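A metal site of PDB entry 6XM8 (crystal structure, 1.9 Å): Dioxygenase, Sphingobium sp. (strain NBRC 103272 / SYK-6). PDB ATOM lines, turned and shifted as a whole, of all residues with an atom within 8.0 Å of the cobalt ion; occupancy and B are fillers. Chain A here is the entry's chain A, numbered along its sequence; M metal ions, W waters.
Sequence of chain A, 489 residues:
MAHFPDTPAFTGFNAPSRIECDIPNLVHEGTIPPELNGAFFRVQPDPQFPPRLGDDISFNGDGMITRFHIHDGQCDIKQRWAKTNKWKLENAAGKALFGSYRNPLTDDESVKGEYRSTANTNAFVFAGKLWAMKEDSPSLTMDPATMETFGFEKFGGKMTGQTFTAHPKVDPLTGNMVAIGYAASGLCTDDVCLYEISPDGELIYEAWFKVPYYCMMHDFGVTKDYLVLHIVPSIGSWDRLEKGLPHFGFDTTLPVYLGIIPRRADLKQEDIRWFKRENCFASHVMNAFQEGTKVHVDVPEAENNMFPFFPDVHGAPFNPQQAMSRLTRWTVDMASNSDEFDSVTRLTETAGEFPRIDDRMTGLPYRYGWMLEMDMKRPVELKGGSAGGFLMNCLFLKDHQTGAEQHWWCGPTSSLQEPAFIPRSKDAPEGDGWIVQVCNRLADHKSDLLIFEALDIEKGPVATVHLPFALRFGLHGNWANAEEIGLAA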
ATOM      1  N   PHE A  59      -8.677   8.174  -0.616  1.00  0.00           N
ATOM      2  CA  PHE A  59      -8.186   9.436  -1.150  1.00  0.00           C
ATOM      3  C   PHE A  59      -9.289  10.401  -1.557  1.00  0.00           C
ATOM      4  O   PHE A  59      -8.985  11.515  -1.998  1.00  0.00           O
ATOM      5  CB  PHE A  59      -7.285   9.213  -2.377  1.00  0.00           C
ATOM      6  CG  PHE A  59      -5.920   8.666  -2.065  1.00  0.00           C
ATOM      7  CD1 PHE A  59      -5.518   8.401  -0.769  1.00  0.00           C
ATOM      8  CD2 PHE A  59      -5.036   8.407  -3.104  1.00  0.00           C
ATOM      9  CE1 PHE A  59      -4.264   7.879  -0.513  1.00  0.00           C
ATOM     10  CE2 PHE A  59      -3.784   7.893  -2.860  1.00  0.00           C
ATOM     11  CZ  PHE A  59      -3.399   7.613  -1.562  1.00  0.00           C
ATOM     12  N   THR A 121      -5.230  16.887   0.725  1.00  0.00           N
ATOM     13  CA  THR A 121      -3.914  16.279   0.560  1.00  0.00           C
ATOM     14  C   THR A 121      -2.784  17.024   1.265  1.00  0.00           C
ATOM     15  O   THR A 121      -1.817  16.390   1.667  1.00  0.00           O
ATOM     16  CB  THR A 121      -3.572  16.159  -0.936  1.00  0.00           C
ATOM     17  OG1 THR A 121      -4.601  15.388  -1.575  1.00  0.00           O
ATOM     18  CG2 THR A 121      -2.238  15.473  -1.158  1.00  0.00           C
ATOM     19  N   ASN A 122      -2.885  18.336   1.444  1.00  0.00           N
ATOM     20  CA  ASN A 122      -1.872  19.060   2.202  1.00  0.00           C
ATOM     21  C   ASN A 122      -2.516  20.212   2.957  1.00  0.00           C
ATOM     22  O   ASN A 122      -3.533  20.758   2.538  1.00  0.00           O
ATOM     23  CB  ASN A 122      -0.738  19.579   1.303  1.00  0.00           C
ATOM     24  CG  ASN A 122       0.585  19.730   2.037  1.00  0.00           C
ATOM     25  OD1 ASN A 122       0.626  19.820   3.260  1.00  0.00           O
ATOM     26  ND2 ASN A 122       1.672  19.759   1.279  1.00  0.00           N
ATOM     27  N   GLU A 135      -4.785  18.289  -5.964  1.00  0.00           N
ATOM     28  CA  GLU A 135      -4.093  18.520  -7.217  1.00  0.00           C
ATOM     29  C   GLU A 135      -5.006  18.572  -8.435  1.00  0.00           C
ATOM     30  O   GLU A 135      -4.492  18.706  -9.554  1.00  0.00           O
ATOM     31  CB  GLU A 135      -3.040  17.437  -7.440  1.00  0.00           C
ATOM     32  CG  GLU A 135      -3.627  16.040  -7.565  1.00  0.00           C
ATOM     33  CD  GLU A 135      -2.623  14.967  -7.212  1.00  0.00           C
ATOM     34  OE1 GLU A 135      -2.102  14.989  -6.073  1.00  0.00           O
ATOM     35  OE2 GLU A 135      -2.353  14.098  -8.070  1.00  0.00           O
ATOM     36  N   ALA A 166      -0.546  19.768  -4.745  1.00  0.00           N
ATOM     37  CA  ALA A 166      -0.618  19.636  -3.295  1.00  0.00           C
ATOM     38  C   ALA A 166       0.767  19.491  -2.674  1.00  0.00           C
ATOM     39  O   ALA A 166       0.871  19.249  -1.467  1.00  0.00           O
ATOM     40  CB  ALA A 166      -1.505  18.455  -2.913  1.00  0.00           C
ATOM     41  N   HIS A 167       1.829  19.654  -3.465  1.00  0.00           N
ATOM     42  CA  HIS A 167       3.204  19.496  -2.973  1.00  0.00           C
ATOM     43  C   HIS A 167       4.058  20.735  -3.265  1.00  0.00           C
ATOM     44  O   HIS A 167       5.131  20.632  -3.850  1.00  0.00           O
ATOM     45  CB  HIS A 167       3.815  18.246  -3.570  1.00  0.00           C
ATOM     46  CG  HIS A 167       3.554  17.004  -2.773  1.00  0.00           C
ATOM     47  ND1 HIS A 167       4.224  16.724  -1.603  1.00  0.00           N
ATOM     48  CD2 HIS A 167       2.695  15.974  -2.972  1.00  0.00           C
ATOM     49  CE1 HIS A 167       3.799  15.564  -1.125  1.00  0.00           C
ATOM     50  NE2 HIS A 167       2.865  15.093  -1.933  1.00  0.00           N
ATOM     51  N   MET A 216      -0.382  10.526 -13.071  1.00  0.00           N
ATOM     52  CA  MET A 216      -0.467  11.201 -11.784  1.00  0.00           C
ATOM     53  C   MET A 216       0.875  11.877 -11.510  1.00  0.00           C
ATOM     54  O   MET A 216       1.848  11.216 -11.144  1.00  0.00           O
ATOM     55  CB  MET A 216      -0.823  10.241 -10.659  1.00  0.00           C
ATOM     56  CG  MET A 216      -1.219  10.962  -9.364  1.00  0.00           C
ATOM     57  SD  MET A 216      -1.147   9.942  -7.879  1.00  0.00           S
ATOM     58  CE  MET A 216      -2.368   8.694  -8.260  1.00  0.00           C
ATOM     59  N   HIS A 218       2.006  13.747  -8.961  1.00  0.00           N
ATOM     60  CA  HIS A 218       1.631  14.068  -7.591  1.00  0.00           C
ATOM     61  C   HIS A 218       2.673  14.954  -6.909  1.00  0.00           C
ATOM     62  O   HIS A 218       2.317  15.903  -6.188  1.00  0.00           O
ATOM     63  CB  HIS A 218       1.417  12.761  -6.812  1.00  0.00           C
ATOM     64  CG  HIS A 218       1.078  12.947  -5.368  1.00  0.00           C
ATOM     65  ND1 HIS A 218      -0.110  13.484  -4.947  1.00  0.00           N
ATOM     66  CD2 HIS A 218       1.783  12.647  -4.245  1.00  0.00           C
ATOM     67  CE1 HIS A 218      -0.136  13.521  -3.625  1.00  0.00           C
ATOM     68  NE2 HIS A 218       1.004  13.023  -3.173  1.00  0.00           N
ATOM     69  N   ASP A 219       3.957  14.673  -7.128  1.00  0.00           N
ATOM     70  CA  ASP A 219       5.047  15.368  -6.476  1.00  0.00           C
ATOM     71  C   ASP A 219       6.094  15.725  -7.522  1.00  0.00           C
ATOM     72  O   ASP A 219       5.977  15.372  -8.703  1.00  0.00           O
ATOM     73  CB  ASP A 219       5.649  14.498  -5.352  1.00  0.00           C
ATOM     74  CG  ASP A 219       6.337  15.316  -4.280  1.00  0.00           C
ATOM     75  OD1 ASP A 219       6.515  16.549  -4.439  1.00  0.00           O
ATOM     76  OD2 ASP A 219       6.703  14.715  -3.244  1.00  0.00           O
ATOM     77  N   SER A 283       6.614   8.027  -6.053  1.00  0.00           N
ATOM     78  CA  SER A 283       5.614   9.062  -5.831  1.00  0.00           C
ATOM     79  C   SER A 283       6.215  10.330  -5.250  1.00  0.00           C
ATOM     80  O   SER A 283       6.156  11.393  -5.870  1.00  0.00           O
ATOM     81  CB  SER A 283       4.513   8.537  -4.890  1.00  0.00           C
ATOM     82  OG  SER A 283       3.533   9.534  -4.672  1.00  0.00           O
ATOM     83  N   HIS A 284       6.833  10.257  -4.073  1.00  0.00           N
ATOM     84  CA  HIS A 284       7.259  11.422  -3.336  1.00  0.00           C
ATOM     85  C   HIS A 284       8.737  11.715  -3.554  1.00  0.00           C
ATOM     86  O   HIS A 284       9.524  10.849  -3.948  1.00  0.00           O
ATOM     87  CB  HIS A 284       6.966  11.229  -1.849  1.00  0.00           C
ATOM     88  CG  HIS A 284       5.517  11.360  -1.517  1.00  0.00           C
ATOM     89  ND1 HIS A 284       4.792  10.381  -0.871  1.00  0.00           N
ATOM     90  CD2 HIS A 284       4.648  12.358  -1.774  1.00  0.00           C
ATOM     91  CE1 HIS A 284       3.541  10.770  -0.740  1.00  0.00           C
ATOM     92  NE2 HIS A 284       3.426  11.979  -1.274  1.00  0.00           N
ATOM     93  N   VAL A 285       9.108  12.965  -3.287  1.00  0.00           N
ATOM     94  CA  VAL A 285      10.462  13.469  -3.431  1.00  0.00           C
ATOM     95  C   VAL A 285      10.937  13.937  -2.061  1.00  0.00           C
ATOM     96  O   VAL A 285      10.333  14.834  -1.457  1.00  0.00           O
ATOM     97  CB  VAL A 285      10.523  14.623  -4.450  1.00  0.00           C
ATOM     98  CG1 VAL A 285      11.891  15.297  -4.408  1.00  0.00           C
ATOM     99  CG2 VAL A 285      10.199  14.124  -5.863  1.00  0.00           C
ATOM    100  N   PHE A 307      -0.319   1.761  -5.271  1.00  0.00           N
ATOM    101  CA  PHE A 307      -1.727   2.089  -5.011  1.00  0.00           C
ATOM    102  C   PHE A 307      -2.614   0.909  -5.379  1.00  0.00           C
ATOM    103  O   PHE A 307      -2.990   0.761  -6.556  1.00  0.00           O
ATOM    104  CB  PHE A 307      -2.164   3.319  -5.807  1.00  0.00           C
ATOM    105  CG  PHE A 307      -1.346   4.555  -5.561  1.00  0.00           C
ATOM    106  CD1 PHE A 307      -1.144   5.031  -4.278  1.00  0.00           C
ATOM    107  CD2 PHE A 307      -0.820   5.255  -6.631  1.00  0.00           C
ATOM    108  CE1 PHE A 307      -0.408   6.177  -4.070  1.00  0.00           C
ATOM    109  CE2 PHE A 307      -0.082   6.391  -6.421  1.00  0.00           C
ATOM    110  CZ  PHE A 307       0.123   6.858  -5.136  1.00  0.00           C
ATOM    111  N   GLU A 353       8.408   5.579   3.363  1.00  0.00           N
ATOM    112  CA  GLU A 353       7.762   6.567   2.513  1.00  0.00           C
ATOM    113  C   GLU A 353       7.584   7.841   3.335  1.00  0.00           C
ATOM    114  O   GLU A 353       8.165   7.984   4.415  1.00  0.00           O
ATOM    115  CB  GLU A 353       6.432   6.018   1.975  1.00  0.00           C
ATOM    116  CG  GLU A 353       6.388   5.908   0.452  1.00  0.00           C
ATOM    117  CD  GLU A 353       6.273   7.261  -0.227  1.00  0.00           C
ATOM    118  OE1 GLU A 353       6.573   7.335  -1.441  1.00  0.00           O
ATOM    119  OE2 GLU A 353       5.886   8.244   0.427  1.00  0.00           O
ATOM    120  N   PHE A 354       6.777   8.770   2.817  1.00  0.00           N
ATOM    121  CA  PHE A 354       6.550  10.054   3.465  1.00  0.00           C
ATOM    122  C   PHE A 354       7.880  10.747   3.797  1.00  0.00           C
ATOM    123  O   PHE A 354       8.119  11.104   4.938  1.00  0.00           O
ATOM    124  CB  PHE A 354       5.698   9.886   4.716  1.00  0.00           C
ATOM    125  CG  PHE A 354       4.210   9.867   4.464  1.00  0.00           C
ATOM    126  CD1 PHE A 354       3.595  10.914   3.788  1.00  0.00           C
ATOM    127  CD2 PHE A 354       3.435   8.824   4.928  1.00  0.00           C
ATOM    128  CE1 PHE A 354       2.221  10.898   3.567  1.00  0.00           C
ATOM    129  CE2 PHE A 354       2.060   8.808   4.707  1.00  0.00           C
ATOM    130  CZ  PHE A 354       1.458   9.847   4.032  1.00  0.00           C
ATOM    131  N   PRO A 355       8.746  10.930   2.807  1.00  0.00           N
ATOM    132  CA  PRO A 355      10.067  11.529   3.093  1.00  0.00           C
ATOM    133  C   PRO A 355       9.968  13.009   3.397  1.00  0.00           C
ATOM    134  O   PRO A 355       9.197  13.742   2.779  1.00  0.00           O
ATOM    135  CB  PRO A 355      10.851  11.275   1.798  1.00  0.00           C
ATOM    136  CG  PRO A 355       9.781  11.310   0.723  1.00  0.00           C
ATOM    137  CD  PRO A 355       8.559  10.662   1.368  1.00  0.00           C
ATOM    138  N   GLU A 418       2.809  11.135   8.888  1.00  0.00           N
ATOM    139  CA  GLU A 418       3.969  11.833   8.325  1.00  0.00           C
ATOM    140  C   GLU A 418       4.642  12.744   9.351  1.00  0.00           C
ATOM    141  O   GLU A 418       3.956  13.562   9.987  1.00  0.00           O
ATOM    142  CB  GLU A 418       3.540  12.659   7.109  1.00  0.00           C
ATOM    143  CG  GLU A 418       4.684  13.409   6.446  1.00  0.00           C
ATOM    144  CD  GLU A 418       4.209  14.485   5.482  1.00  0.00           C
ATOM    145  OE1 GLU A 418       3.477  15.384   5.922  1.00  0.00           O
ATOM    146  OE2 GLU A 418       4.585  14.425   4.292  1.00  0.00           O
ATOM    147  N   LEU A 475      -2.632  12.833   5.308  1.00  0.00           N
ATOM    148  CA  LEU A 475      -1.674  13.013   4.218  1.00  0.00           C
ATOM    149  C   LEU A 475      -0.589  13.953   4.719  1.00  0.00           C
ATOM    150  O   LEU A 475       0.158  13.589   5.640  1.00  0.00           O
ATOM    151  CB  LEU A 475      -2.379  13.500   2.963  1.00  0.00           C
ATOM    152  CG  LEU A 475      -3.127  12.385   2.212  1.00  0.00           C
ATOM    153  CD1 LEU A 475      -2.231  11.209   1.799  1.00  0.00           C
ATOM    154  CD2 LEU A 475      -4.314  11.860   3.030  1.00  0.00           C
ATOM    155  N   HIS A 476      -0.489  15.167   4.187  1.00  0.00           N
ATOM    156  CA  HIS A 476       0.681  15.994   4.444  1.00  0.00           C
ATOM    157  C   HIS A 476       0.412  17.151   5.396  1.00  0.00           C
ATOM    158  O   HIS A 476      -0.726  17.623   5.535  1.00  0.00           O
ATOM    159  CB  HIS A 476       1.239  16.502   3.122  1.00  0.00           C
ATOM    160  CG  HIS A 476       1.596  15.400   2.173  1.00  0.00           C
ATOM    161  ND1 HIS A 476       2.623  14.516   2.434  1.00  0.00           N
ATOM    162  CD2 HIS A 476       1.045  15.009   1.003  1.00  0.00           C
ATOM    163  CE1 HIS A 476       2.705  13.640   1.444  1.00  0.00           C
ATOM    164  NE2 HIS A 476       1.755  13.918   0.573  1.00  0.00           N
HETATM  165 CO    CO M   1       1.928  13.356  -1.359  1.00  0.00          CO
HETATM  166  O   HOH W   1       0.422  11.870  -0.783  1.00  0.00           O
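The backbone NH (N) of His 476 sits at hydrogen-bond distance from the backbone carbonyl oxygen (O) of Thr 121 (3.1 Å).
A ring nitrogen (ND1) of His 476 sits at hydrogen-bond distance from the side-chain carboxylate (OE2) of Glu 418.
The side-chain amide oxygen (OD1) of Asn 122 sits close to the backbone carbonyl oxygen (O) of His 476, 3.4 Å away.
ND1 of His 284 is in hydrogen-bond range of OE2 of Glu 353 (2.7 Å).
OE1 of Glu 135 lies within hydrogen-bond range of ND1 of His 218, at 2.7 Å.
Within 4 Å of the cobalt ion: His 167, His 218, His 284 and His 476.
The cobalt ion is bound by a ring nitrogen (NE2) of His 476 (2.0 Å), a ring nitrogen (NE2) of His 284 (2.0 Å), a ring nitrogen (NE2) of His 167 (2.1 Å), a ring nitrogen (NE2) of His 218 (2.1 Å) and water W1 (2.2 Å).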
